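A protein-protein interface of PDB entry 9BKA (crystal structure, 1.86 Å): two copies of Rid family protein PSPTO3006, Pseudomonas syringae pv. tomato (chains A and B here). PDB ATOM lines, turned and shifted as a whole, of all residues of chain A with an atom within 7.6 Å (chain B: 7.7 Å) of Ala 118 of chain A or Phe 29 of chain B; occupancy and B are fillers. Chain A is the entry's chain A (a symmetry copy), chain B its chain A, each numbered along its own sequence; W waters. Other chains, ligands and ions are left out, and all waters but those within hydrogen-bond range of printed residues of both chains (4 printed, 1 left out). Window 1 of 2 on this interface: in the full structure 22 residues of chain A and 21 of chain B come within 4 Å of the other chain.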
ATOM      1  N   PRO A  14      23.531   3.441  29.587  1.00  0.00           N
ATOM      2  CA  PRO A  14      22.401   2.504  29.650  1.00  0.00           C
ATOM      3  C   PRO A  14      21.235   2.889  28.750  1.00  0.00           C
ATOM      4  O   PRO A  14      20.091   2.590  29.092  1.00  0.00           O
ATOM      5  CB  PRO A  14      21.998   2.556  31.129  1.00  0.00           C
ATOM      6  CG  PRO A  14      22.343   3.956  31.535  1.00  0.00           C
ATOM      7  CD  PRO A  14      23.609   4.289  30.791  1.00  0.00           C
ATOM      8  N   ILE A  15      21.488   3.536  27.604  1.00  0.00           N
ATOM      9  CA  ILE A  15      20.426   3.927  26.681  1.00  0.00           C
ATOM     10  C   ILE A  15      20.836   3.587  25.251  1.00  0.00           C
ATOM     11  O   ILE A  15      22.020   3.475  24.926  1.00  0.00           O
ATOM     12  CB  ILE A  15      20.066   5.433  26.784  1.00  0.00           C
ATOM     13  CG1 ILE A  15      21.058   6.303  26.004  1.00  0.00           C
ATOM     14  CG2 ILE A  15      20.005   5.894  28.249  1.00  0.00           C
ATOM     15  CD1 ILE A  15      20.728   7.795  26.072  1.00  0.00           C
ATOM     16  N   SER A  16      19.835   3.422  24.388  1.00  0.00           N
ATOM     17  CA  SER A  16      20.094   3.249  22.965  1.00  0.00           C
ATOM     18  C   SER A  16      20.094   4.608  22.278  1.00  0.00           C
ATOM     19  O   SER A  16      19.184   5.421  22.482  1.00  0.00           O
ATOM     20  CB  SER A  16      19.056   2.335  22.318  1.00  0.00           C
ATOM     21  OG  SER A  16      19.248   0.987  22.700  1.00  0.00           O
ATOM     22  N   GLN A  17      21.116   4.851  21.462  1.00  0.00           N
ATOM     23  CA  GLN A  17      21.154   6.083  20.683  1.00  0.00           C
ATOM     24  C   GLN A  17      19.944   6.183  19.762  1.00  0.00           C
ATOM     25  O   GLN A  17      19.317   7.245  19.657  1.00  0.00           O
ATOM     26  CB  GLN A  17      22.463   6.134  19.900  1.00  0.00           C
ATOM     27  CG  GLN A  17      22.636   7.288  18.951  1.00  0.00           C
ATOM     28  CD  GLN A  17      23.835   7.052  18.041  1.00  0.00           C
ATOM     29  OE1 GLN A  17      24.888   7.658  18.220  1.00  0.00           O
ATOM     30  NE2 GLN A  17      23.683   6.141  17.076  1.00  0.00           N
ATOM     31  N   THR A  18      19.588   5.086  19.094  1.00  0.00           N
ATOM     32  CA  THR A  18      18.367   5.033  18.308  1.00  0.00           C
ATOM     33  C   THR A  18      17.683   3.697  18.544  1.00  0.00           C
ATOM     34  O   THR A  18      18.331   2.701  18.868  1.00  0.00           O
ATOM     35  CB  THR A  18      18.606   5.208  16.796  1.00  0.00           C
ATOM     36  OG1 THR A  18      19.247   4.036  16.268  1.00  0.00           O
ATOM     37  CG2 THR A  18      19.460   6.421  16.511  1.00  0.00           C
ATOM     38  N   VAL A  19      16.366   3.684  18.366  1.00  0.00           N
ATOM     39  CA  VAL A  19      15.568   2.461  18.386  1.00  0.00           C
ATOM     40  C   VAL A  19      14.668   2.478  17.163  1.00  0.00           C
ATOM     41  O   VAL A  19      13.893   3.424  16.971  1.00  0.00           O
ATOM     42  CB  VAL A  19      14.734   2.326  19.668  1.00  0.00           C
ATOM     43  CG1 VAL A  19      13.844   1.081  19.601  1.00  0.00           C
ATOM     44  CG2 VAL A  19      15.637   2.284  20.900  1.00  0.00           C
ATOM     45  N   THR A  20      14.767   1.438  16.332  1.00  0.00           N
ATOM     46  CA  THR A  20      13.938   1.319  15.143  1.00  0.00           C
ATOM     47  C   THR A  20      12.760   0.397  15.424  1.00  0.00           C
ATOM     48  O   THR A  20      12.928  -0.686  15.997  1.00  0.00           O
ATOM     49  CB  THR A  20      14.750   0.798  13.953  1.00  0.00           C
ATOM     50  OG1 THR A  20      15.810   1.717  13.675  1.00  0.00           O
ATOM     51  CG2 THR A  20      13.861   0.673  12.723  1.00  0.00           C
ATOM     52  N   VAL A  21      11.574   0.828  15.018  1.00  0.00           N
ATOM     53  CA  VAL A  21      10.324   0.099  15.202  1.00  0.00           C
ATOM     54  C   VAL A  21       9.815  -0.327  13.830  1.00  0.00           C
ATOM     55  O   VAL A  21       9.577   0.534  12.973  1.00  0.00           O
ATOM     56  CB  VAL A  21       9.271   0.956  15.920  1.00  0.00           C
ATOM     57  CG1 VAL A  21       7.966   0.166  16.078  1.00  0.00           C
ATOM     58  CG2 VAL A  21       9.808   1.429  17.257  1.00  0.00           C
ATOM     59  N   LEU A  27       1.975   0.762  18.105  1.00  0.00           N
ATOM     60  CA  LEU A  27       2.540   1.636  19.125  1.00  0.00           C
ATOM     61  C   LEU A  27       1.552   1.785  20.272  1.00  0.00           C
ATOM     62  O   LEU A  27       0.337   1.830  20.054  1.00  0.00           O
ATOM     63  CB  LEU A  27       2.879   3.009  18.546  1.00  0.00           C
ATOM     64  CG  LEU A  27       4.006   3.055  17.517  1.00  0.00           C
ATOM     65  CD1 LEU A  27       4.192   4.478  17.012  1.00  0.00           C
ATOM     66  CD2 LEU A  27       5.291   2.519  18.145  1.00  0.00           C
ATOM     67  N   PHE A  29       1.121   4.466  23.391  1.00  0.00           N
ATOM     68  CA  PHE A  29       1.542   5.712  24.015  1.00  0.00           C
ATOM     69  C   PHE A  29       1.097   5.698  25.473  1.00  0.00           C
ATOM     70  O   PHE A  29      -0.049   5.357  25.766  1.00  0.00           O
ATOM     71  CB  PHE A  29       0.942   6.910  23.264  1.00  0.00           C
ATOM     72  CG  PHE A  29       1.480   7.080  21.859  1.00  0.00           C
ATOM     73  CD1 PHE A  29       0.892   6.423  20.788  1.00  0.00           C
ATOM     74  CD2 PHE A  29       2.587   7.883  21.622  1.00  0.00           C
ATOM     75  CE1 PHE A  29       1.402   6.568  19.491  1.00  0.00           C
ATOM     76  CE2 PHE A  29       3.107   8.034  20.338  1.00  0.00           C
ATOM     77  CZ  PHE A  29       2.512   7.376  19.267  1.00  0.00           C
ATOM     78  N   ILE A  78       9.401  -0.965  25.763  1.00  0.00           N
ATOM     79  CA  ILE A  78       9.521   0.486  25.630  1.00  0.00           C
ATOM     80  C   ILE A  78      10.562   0.820  24.565  1.00  0.00           C
ATOM     81  O   ILE A  78      11.692   0.312  24.580  1.00  0.00           O
ATOM     82  CB  ILE A  78       9.867   1.125  26.983  1.00  0.00           C
ATOM     83  CG1 ILE A  78       8.729   0.905  27.987  1.00  0.00           C
ATOM     84  CG2 ILE A  78      10.166   2.640  26.829  1.00  0.00           C
ATOM     85  CD1 ILE A  78       9.066   1.332  29.387  1.00  0.00           C
ATOM     86  N   VAL A  79      10.183   1.676  23.623  1.00  0.00           N
ATOM     87  CA  VAL A  79      11.104   2.129  22.602  1.00  0.00           C
ATOM     88  C   VAL A  79      11.569   3.559  22.837  1.00  0.00           C
ATOM     89  O   VAL A  79      12.681   3.901  22.422  1.00  0.00           O
ATOM     90  CB  VAL A  79      10.515   1.971  21.184  1.00  0.00           C
ATOM     91  CG1 VAL A  79      10.204   0.497  20.895  1.00  0.00           C
ATOM     92  CG2 VAL A  79       9.287   2.819  21.008  1.00  0.00           C
ATOM     93  N   GLN A  80      10.779   4.395  23.525  1.00  0.00           N
ATOM     94  CA  GLN A  80      11.236   5.747  23.836  1.00  0.00           C
ATOM     95  C   GLN A  80      10.785   6.152  25.235  1.00  0.00           C
ATOM     96  O   GLN A  80       9.641   5.907  25.620  1.00  0.00           O
ATOM     97  CB  GLN A  80      10.704   6.743  22.793  1.00  0.00           C
ATOM     98  CG  GLN A  80      10.873   8.204  23.173  1.00  0.00           C
ATOM     99  CD  GLN A  80      10.257   9.113  22.144  1.00  0.00           C
ATOM    100  OE1 GLN A  80       9.035   9.320  22.124  1.00  0.00           O
ATOM    101  NE2 GLN A  80      11.094   9.662  21.266  1.00  0.00           N
ATOM    102  N   LEU A  81      11.691   6.777  25.984  1.00  0.00           N
ATOM    103  CA  LEU A  81      11.439   7.226  27.346  1.00  0.00           C
ATOM    104  C   LEU A  81      11.783   8.692  27.441  1.00  0.00           C
ATOM    105  O   LEU A  81      12.836   9.116  26.960  1.00  0.00           O
ATOM    106  CB  LEU A  81      12.305   6.491  28.376  1.00  0.00           C
ATOM    107  CG  LEU A  81      11.839   5.194  29.006  1.00  0.00           C
ATOM    108  CD1 LEU A  81      12.904   4.759  30.009  1.00  0.00           C
ATOM    109  CD2 LEU A  81      10.499   5.413  29.682  1.00  0.00           C
ATOM    110  N   ARG A  82      10.922   9.465  28.083  1.00  0.00           N
ATOM    111  CA  ARG A  82      11.222  10.866  28.338  1.00  0.00           C
ATOM    112  C   ARG A  82      11.098  11.113  29.833  1.00  0.00           C
ATOM    113  O   ARG A  82      10.057  10.812  30.417  1.00  0.00           O
ATOM    114  CB  ARG A  82      10.280  11.779  27.551  1.00  0.00           C
ATOM    115  CG  ARG A  82      10.680  13.231  27.558  1.00  0.00           C
ATOM    116  CD  ARG A  82       9.914  14.003  26.492  1.00  0.00           C
ATOM    117  NE  ARG A  82      10.171  13.434  25.178  1.00  0.00           N
ATOM    118  CZ  ARG A  82       9.351  12.595  24.564  1.00  0.00           C
ATOM    119  NH1 ARG A  82       8.169  12.293  25.074  1.00  0.00           N
ATOM    120  NH2 ARG A  82       9.736  12.035  23.422  1.00  0.00           N
ATOM    121  N   TYR A 104      17.375   4.118  37.491  1.00  0.00           N
ATOM    122  CA  TYR A 104      17.149   3.723  36.111  1.00  0.00           C
ATOM    123  C   TYR A 104      17.908   2.456  35.752  1.00  0.00           C
ATOM    124  O   TYR A 104      17.376   1.572  35.073  1.00  0.00           O
ATOM    125  CB  TYR A 104      17.592   4.868  35.219  1.00  0.00           C
ATOM    126  CG  TYR A 104      17.331   4.627  33.771  1.00  0.00           C
ATOM    127  CD1 TYR A 104      16.105   4.968  33.209  1.00  0.00           C
ATOM    128  CD2 TYR A 104      18.315   4.096  32.950  1.00  0.00           C
ATOM    129  CE1 TYR A 104      15.861   4.772  31.872  1.00  0.00           C
ATOM    130  CE2 TYR A 104      18.073   3.889  31.620  1.00  0.00           C
ATOM    131  CZ  TYR A 104      16.848   4.227  31.088  1.00  0.00           C
ATOM    132  OH  TYR A 104      16.568   4.051  29.762  1.00  0.00           O
ATOM    133  N   LYS A 116      17.277  -1.549  26.156  1.00  0.00           N
ATOM    134  CA  LYS A 116      17.504  -0.155  26.522  1.00  0.00           C
ATOM    135  C   LYS A 116      16.795   0.740  25.517  1.00  0.00           C
ATOM    136  O   LYS A 116      17.156   0.728  24.323  1.00  0.00           O
ATOM    137  CB  LYS A 116      19.001   0.150  26.570  1.00  0.00           C
ATOM    138  CG  LYS A 116      19.748  -0.647  27.621  1.00  0.00           C
ATOM    139  CD  LYS A 116      21.229  -0.278  27.655  1.00  0.00           C
ATOM    140  CE  LYS A 116      22.051  -1.108  26.684  1.00  0.00           C
ATOM    141  NZ  LYS A 116      23.341  -1.547  27.310  1.00  0.00           N
ATOM    142  N   PRO A 117      15.792   1.510  25.930  1.00  0.00           N
ATOM    143  CA  PRO A 117      15.103   2.401  24.992  1.00  0.00           C
ATOM    144  C   PRO A 117      15.941   3.636  24.699  1.00  0.00           C
ATOM    145  O   PRO A 117      16.944   3.921  25.362  1.00  0.00           O
ATOM    146  CB  PRO A 117      13.824   2.782  25.741  1.00  0.00           C
ATOM    147  CG  PRO A 117      14.256   2.782  27.169  1.00  0.00           C
ATOM    148  CD  PRO A 117      15.242   1.623  27.292  1.00  0.00           C
ATOM    149  N   ALA A 118      15.529   4.340  23.648  1.00  0.00           N
ATOM    150  CA  ALA A 118      15.972   5.708  23.455  1.00  0.00           C
ATOM    151  C   ALA A 118      15.432   6.548  24.604  1.00  0.00           C
ATOM    152  O   ALA A 118      14.327   6.311  25.099  1.00  0.00           O
ATOM    153  CB  ALA A 118      15.479   6.243  22.113  1.00  0.00           C
ATOM    154  N   ARG A 119      16.220   7.518  25.052  1.00  0.00           N
ATOM    155  CA  ARG A 119      15.837   8.283  26.224  1.00  0.00           C
ATOM    156  C   ARG A 119      16.226   9.746  26.061  1.00  0.00           C
ATOM    157  O   ARG A 119      17.229  10.075  25.423  1.00  0.00           O
ATOM    158  CB  ARG A 119      16.496   7.713  27.484  1.00  0.00           C
ATOM    159  CG  ARG A 119      15.960   8.310  28.784  1.00  0.00           C
ATOM    160  CD  ARG A 119      16.707   7.767  29.978  1.00  0.00           C
ATOM    161  NE  ARG A 119      17.950   8.493  30.213  1.00  0.00           N
ATOM    162  CZ  ARG A 119      18.723   8.310  31.274  1.00  0.00           C
ATOM    163  NH1 ARG A 119      18.406   7.435  32.215  1.00  0.00           N
ATOM    164  NH2 ARG A 119      19.838   9.024  31.397  1.00  0.00           N
ATOM    165  N   THR A 120      15.417  10.616  26.657  1.00  0.00           N
ATOM    166  CA  THR A 120      15.747  12.020  26.863  1.00  0.00           C
ATOM    167  C   THR A 120      15.433  12.344  28.313  1.00  0.00           C
ATOM    168  O   THR A 120      14.401  11.905  28.829  1.00  0.00           O
ATOM    169  CB  THR A 120      14.944  12.951  25.927  1.00  0.00           C
ATOM    170  OG1 THR A 120      15.245  12.643  24.555  1.00  0.00           O
ATOM    171  CG2 THR A 120      15.313  14.401  26.190  1.00  0.00           C
ATOM    172  N   GLU A 137       7.407   9.688  30.690  1.00  0.00           N
ATOM    173  CA  GLU A 137       6.521   9.477  29.557  1.00  0.00           C
ATOM    174  C   GLU A 137       7.116   8.363  28.700  1.00  0.00           C
ATOM    175  O   GLU A 137       8.337   8.233  28.612  1.00  0.00           O
ATOM    176  CB  GLU A 137       6.419  10.797  28.762  1.00  0.00           C
ATOM    177  CG  GLU A 137       5.314  10.903  27.783  1.00  0.00           C
ATOM    178  CD  GLU A 137       5.339  12.253  27.101  1.00  0.00           C
ATOM    179  OE1 GLU A 137       6.321  13.019  27.326  1.00  0.00           O
ATOM    180  OE2 GLU A 137       4.392  12.553  26.354  1.00  0.00           O
ATOM    181  N   VAL A 139       6.792   5.521  25.090  1.00  0.00           N
ATOM    182  CA  VAL A 139       6.166   4.845  23.960  1.00  0.00           C
ATOM    183  C   VAL A 139       6.728   3.433  23.902  1.00  0.00           C
ATOM    184  O   VAL A 139       7.946   3.231  24.022  1.00  0.00           O
ATOM    185  CB  VAL A 139       6.391   5.564  22.616  1.00  0.00           C
ATOM    186  CG1 VAL A 139       5.675   4.807  21.519  1.00  0.00           C
ATOM    187  CG2 VAL A 139       5.872   6.987  22.680  1.00  0.00           C
ATOM    188  N   ALA A 140       5.822   2.465  23.730  1.00  0.00           N
ATOM    189  CA  ALA A 140       6.136   1.046  23.676  1.00  0.00           C
ATOM    190  C   ALA A 140       5.651   0.498  22.342  1.00  0.00           C
ATOM    191  O   ALA A 140       4.857   1.133  21.648  1.00  0.00           O
ATOM    192  CB  ALA A 140       5.482   0.292  24.840  1.00  0.00           C
ATOM    193  N   ALA A 141       6.144  -0.679  21.962  1.00  0.00           N
ATOM    194  CA  ALA A 141       5.739  -1.283  20.703  1.00  0.00           C
ATOM    195  C   ALA A 141       5.366  -2.741  20.928  1.00  0.00           C
ATOM    196  O   ALA A 141       6.009  -3.446  21.712  1.00  0.00           O
ATOM    197  CB  ALA A 141       6.846  -1.179  19.642  1.00  0.00           C
ATOM    198  N   SER B  26       8.648   2.614   8.707  1.00  0.00           N
ATOM    199  CA  SER B  26       9.177   2.297  10.024  1.00  0.00           C
ATOM    200  C   SER B  26       9.622   3.575  10.723  1.00  0.00           C
ATOM    201  O   SER B  26      10.123   4.505  10.088  1.00  0.00           O
ATOM    202  CB  SER B  26      10.355   1.333   9.924  1.00  0.00           C
ATOM    203  OG  SER B  26       9.918   0.071   9.458  1.00  0.00           O
ATOM    204  N   LEU B  27       9.442   3.619  12.036  1.00  0.00           N
ATOM    205  CA  LEU B  27       9.859   4.774  12.818  1.00  0.00           C
ATOM    206  C   LEU B  27      11.204   4.490  13.469  1.00  0.00           C
ATOM    207  O   LEU B  27      11.476   3.358  13.886  1.00  0.00           O
ATOM    208  CB  LEU B  27       8.824   5.119  13.887  1.00  0.00           C
ATOM    209  CG  LEU B  27       7.472   5.623  13.390  1.00  0.00           C
ATOM    210  CD1 LEU B  27       6.545   5.880  14.569  1.00  0.00           C
ATOM    211  CD2 LEU B  27       7.674   6.888  12.559  1.00  0.00           C
ATOM    212  N   ILE B  28      12.041   5.523  13.555  1.00  0.00           N
ATOM    213  CA  ILE B  28      13.310   5.477  14.274  1.00  0.00           C
ATOM    214  C   ILE B  28      13.262   6.576  15.330  1.00  0.00           C
ATOM    215  O   ILE B  28      13.160   7.767  14.999  1.00  0.00           O
ATOM    216  CB  ILE B  28      14.533   5.669  13.355  1.00  0.00           C
ATOM    217  CG1 ILE B  28      14.532   4.673  12.196  1.00  0.00           C
ATOM    218  CG2 ILE B  28      15.824   5.558  14.151  1.00  0.00           C
ATOM    219  CD1 ILE B  28      13.717   5.141  10.994  1.00  0.00           C
ATOM    220  N   PHE B  29      13.323   6.176  16.594  1.00  0.00           N
ATOM    221  CA  PHE B  29      13.343   7.114  17.708  1.00  0.00           C
ATOM    222  C   PHE B  29      14.795   7.400  18.074  1.00  0.00           C
ATOM    223  O   PHE B  29      15.597   6.473  18.189  1.00  0.00           O
ATOM    224  CB  PHE B  29      12.576   6.533  18.903  1.00  0.00           C
ATOM    225  CG  PHE B  29      11.088   6.388  18.659  1.00  0.00           C
ATOM    226  CD1 PHE B  29      10.570   5.240  18.079  1.00  0.00           C
ATOM    227  CD2 PHE B  29      10.216   7.416  18.995  1.00  0.00           C
ATOM    228  CE1 PHE B  29       9.195   5.114  17.838  1.00  0.00           C
ATOM    229  CE2 PHE B  29       8.847   7.305  18.759  1.00  0.00           C
ATOM    230  CZ  PHE B  29       8.333   6.151  18.179  1.00  0.00           C
ATOM    231  N   ILE B  30      15.138   8.673  18.264  1.00  0.00           N
ATOM    232  CA  ILE B  30      16.514   9.070  18.538  1.00  0.00           C
ATOM    233  C   ILE B  30      16.574   9.708  19.917  1.00  0.00           C
ATOM    234  O   ILE B  30      15.784  10.611  20.232  1.00  0.00           O
ATOM    235  CB  ILE B  30      17.044  10.034  17.462  1.00  0.00           C
ATOM    236  CG1 ILE B  30      16.766   9.452  16.073  1.00  0.00           C
ATOM    237  CG2 ILE B  30      18.530  10.329  17.691  1.00  0.00           C
ATOM    238  CD1 ILE B  30      17.110  10.383  14.913  1.00  0.00           C
ATOM    239  N   SER B  31      17.510   9.235  20.731  1.00  0.00           N
ATOM    240  CA  SER B  31      17.706   9.770  22.066  1.00  0.00           C
ATOM    241  C   SER B  31      18.090  11.240  22.006  1.00  0.00           C
ATOM    242  O   SER B  31      18.589  11.739  20.993  1.00  0.00           O
ATOM    243  CB  SER B  31      18.801   8.997  22.793  1.00  0.00           C
ATOM    244  OG  SER B  31      18.331   7.725  23.168  1.00  0.00           O
ATOM    245  N   GLY B  32      17.863  11.930  23.126  1.00  0.00           N
ATOM    246  CA  GLY B  32      18.258  13.314  23.270  1.00  0.00           C
ATOM    247  C   GLY B  32      19.712  13.512  22.899  1.00  0.00           C
ATOM    248  O   GLY B  32      20.594  12.781  23.364  1.00  0.00           O
ATOM    249  N   ILE B  67      24.294  10.497  13.096  1.00  0.00           N
ATOM    250  CA  ILE B  67      23.521   9.395  13.671  1.00  0.00           C
ATOM    251  C   ILE B  67      22.626   8.775  12.607  1.00  0.00           C
ATOM    252  O   ILE B  67      22.553   7.548  12.461  1.00  0.00           O
ATOM    253  CB  ILE B  67      22.701   9.882  14.881  1.00  0.00           C
ATOM    254  CG1 ILE B  67      23.621  10.257  16.044  1.00  0.00           C
ATOM    255  CG2 ILE B  67      21.708   8.807  15.305  1.00  0.00           C
ATOM    256  CD1 ILE B  67      22.919  10.980  17.192  1.00  0.00           C
ATOM    257  N   GLN B  80       9.694  14.501  13.301  1.00  0.00           N
ATOM    258  CA  GLN B  80       9.395  15.349  14.451  1.00  0.00           C
ATOM    259  C   GLN B  80      10.678  15.699  15.199  1.00  0.00           C
ATOM    260  O   GLN B  80      11.532  14.840  15.417  1.00  0.00           O
ATOM    261  CB  GLN B  80       8.404  14.646  15.391  1.00  0.00           C
ATOM    262  CG  GLN B  80       8.246  15.305  16.751  1.00  0.00           C
ATOM    263  CD  GLN B  80       7.325  14.515  17.640  1.00  0.00           C
ATOM    264  OE1 GLN B  80       7.724  13.508  18.239  1.00  0.00           O
ATOM    265  NE2 GLN B  80       6.073  14.959  17.730  1.00  0.00           N
ATOM    266  N   GLU B 137      15.741  16.132  20.477  1.00  0.00           N
ATOM    267  CA  GLU B 137      15.156  14.804  20.401  1.00  0.00           C
ATOM    268  C   GLU B 137      14.497  14.660  19.031  1.00  0.00           C
ATOM    269  O   GLU B 137      13.982  15.636  18.487  1.00  0.00           O
ATOM    270  CB  GLU B 137      14.119  14.659  21.536  1.00  0.00           C
ATOM    271  CG  GLU B 137      13.664  13.286  21.852  1.00  0.00           C
ATOM    272  CD  GLU B 137      12.668  13.308  22.989  1.00  0.00           C
ATOM    273  OE1 GLU B 137      12.258  14.432  23.406  1.00  0.00           O
ATOM    274  OE2 GLU B 137      12.297  12.224  23.470  1.00  0.00           O
ATOM    275  N   ALA B 138      14.507  13.462  18.445  1.00  0.00           N
ATOM    276  CA  ALA B 138      13.921  13.392  17.110  1.00  0.00           C
ATOM    277  C   ALA B 138      13.261  12.043  16.851  1.00  0.00           C
ATOM    278  O   ALA B 138      13.606  11.021  17.454  1.00  0.00           O
ATOM    279  CB  ALA B 138      14.961  13.677  16.028  1.00  0.00           C
ATOM    280  N   VAL B 139      12.291  12.063  15.933  1.00  0.00           N
ATOM    281  CA  VAL B 139      11.744  10.850  15.338  1.00  0.00           C
ATOM    282  C   VAL B 139      11.883  10.977  13.830  1.00  0.00           C
ATOM    283  O   VAL B 139      11.570  12.029  13.251  1.00  0.00           O
ATOM    284  CB  VAL B 139      10.272  10.593  15.719  1.00  0.00           C
ATOM    285  CG1 VAL B 139       9.811   9.299  15.084  1.00  0.00           C
ATOM    286  CG2 VAL B 139      10.118  10.509  17.224  1.00  0.00           C
ATOM    287  N   ALA B 140      12.365   9.896  13.208  1.00  0.00           N
ATOM    288  CA  ALA B 140      12.605   9.811  11.777  1.00  0.00           C
ATOM    289  C   ALA B 140      11.787   8.653  11.221  1.00  0.00           C
ATOM    290  O   ALA B 140      11.307   7.803  11.969  1.00  0.00           O
ATOM    291  CB  ALA B 140      14.097   9.610  11.480  1.00  0.00           C
ATOM    292  N   ALA B 141      11.604   8.629   9.903  1.00  0.00           N
ATOM    293  CA  ALA B 141      10.836   7.561   9.280  1.00  0.00           C
ATOM    294  C   ALA B 141      11.600   7.008   8.087  1.00  0.00           C
ATOM    295  O   ALA B 141      12.239   7.755   7.340  1.00  0.00           O
ATOM    296  CB  ALA B 141       9.447   8.048   8.837  1.00  0.00           C
HETATM  297  O   HOH W   1      13.934  10.349  22.954  1.00  0.00           O
HETATM  298  O   HOH W   2       6.770   1.940  13.238  1.00  0.00           O
HETATM  299  O   HOH W   3      10.256  12.405  19.910  1.00  0.00           O
HETATM  300  O   HOH W   4      20.286  11.322  25.809  1.00  0.00           O
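Water W4 bridges the backbone carbonyl oxygen of Gly 32 of chain B (2.9 Å) and the backbone carbonyl oxygen of Arg 119 of chain A (3.3 Å). Water W3 lies within hydrogen-bond range of the side-chain amide nitrogen of Gln 80 of chain A (3.2 Å) and the side-chain amide oxygen of Gln 80 of chain B (3.2 Å).
Leu 27 of chain B touches its own counterpart, Leu 27 of chain A. Gln 80 of chain A touches Glu 137 of chain B, but with the chains exchanged Glu 137 of chain A does not touch Gln 80 of chain B (8.8 Å). Positions printed for both chains: 27, 29, 80, 137, 139, 140 and 141. Of the 27 pairs that touch across the chains among the printed residues, 1 has its exchanged pair printed and touching as well.
O of Leu 27 of chain B lies within hydrogen-bond range of N of Val 21 of chain A (2.8 Å). O of Val 19 of chain A lies within hydrogen-bond range of N of Phe 29 of chain B, at 2.8 Å. The side-chain hydroxyl of Ser 31 of chain B is in hydrogen-bond range of the backbone carbonyl oxygen of Ser 16 of chain A. N of Ser 31 of chain B lies within hydrogen-bond range of O of Gln 17 of chain A (2.9 Å). The side-chain hydroxyl (OG) of Ser 31 of chain B sits at hydrogen-bond distance from the backbone NH (N) of Arg 119 of chain A, 2.8 Å away. The backbone carbonyl oxygen of Arg 119 of chain A lies within hydrogen-bond range of the backbone NH of Gly 32 of chain B, at 3.0 Å. The side-chain hydroxyl of Thr 120 of chain A lies within hydrogen-bond range of the backbone NH of Gly 32 of chain B (3.1 Å). The side-chain carboxylate of Glu 137 of chain B lies within salt-bridge range of the guanidinium group of Arg 82 of chain A (2.6 Å). OE2 of Glu 137 of chain B lies close to OG1 of Thr 120 of chain A (3.2 Å).
Ala 118 of chain A touches two residues of chain B. Printed residues of chain A within 4 Å of Phe 29 of chain B: Thr 18 (3.1 Å), Val 19 (2.8 Å), Val 21 (3.8 Å), Val 79 (3.9 Å), Gln 80 (3.3 Å) and Ala 118 (3.9 Å). Of the printed residues of chain B, Gln 80 of chain A touches Phe 29 and Glu 137. Printed residues of chain A within 4 Å of Ser 26 of chain B: Val 21 (3.2 Å). The nearest residue of chain B that does not touch Ala 118 of chain A is Ile 30 of chain B (4.2 Å). The nearest printed residue of chain A that does not touch Glu 137 of chain B is Leu 81 of chain A (4.7 Å).
The backbone NH of Ile 30 of chain B sits at hydrogen-bond distance from the backbone carbonyl oxygen of Ala 138 of chain B, 2.9 Å away. O of Lys 116 of chain A sits at hydrogen-bond distance from OG of Ser 16 of chain A (2.7 Å). The backbone carbonyl oxygen (O) of Val 139 of chain A lies within hydrogen-bond range of the backbone NH (N) of Val 79 of chain A (2.8 Å). N of Thr 120 of chain A lies within hydrogen-bond range of O of Leu 81 of chain A (3.0 Å).
Of the 14 printed residues of chain B, 9 touch a printed residue of chain A. Hydrophobic or aromatic side chains of chain B within 4 Å of the printed part of chain A: Leu 27, Ile 28, Phe 29, Ile 30 and Ile 67. Hydrophobic or aromatic side chains of chain A that line the printed part of chain B: Ile 15, Val 21, Leu 27, Val 79 and Ala 118. Among the printed residues, 27 pairs touch across the chains.
Gln 17 of chain A touches Ile 30 of chain B. CG1 of Ile 67 of chain B touches OE1 of Gln 17 of chain A, at 3.6 Å. Thr 18 of chain A touches Phe 29 of chain B (CA to O, 3.1 Å). Ile 28 of chain B touches Val 19 of chain A (CA to O, 3.4 Å). Val 21 of chain A touches Ser 26 of chain B (O to CB, 3.2 Å). Phe 29 of chain B touches Gln 80 of chain A (CD2 to NE2, 3.3 Å). Gln 80 of chain A touches Glu 137 of chain B. Ser 31 of chain B touches Ala 118 of chain A.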
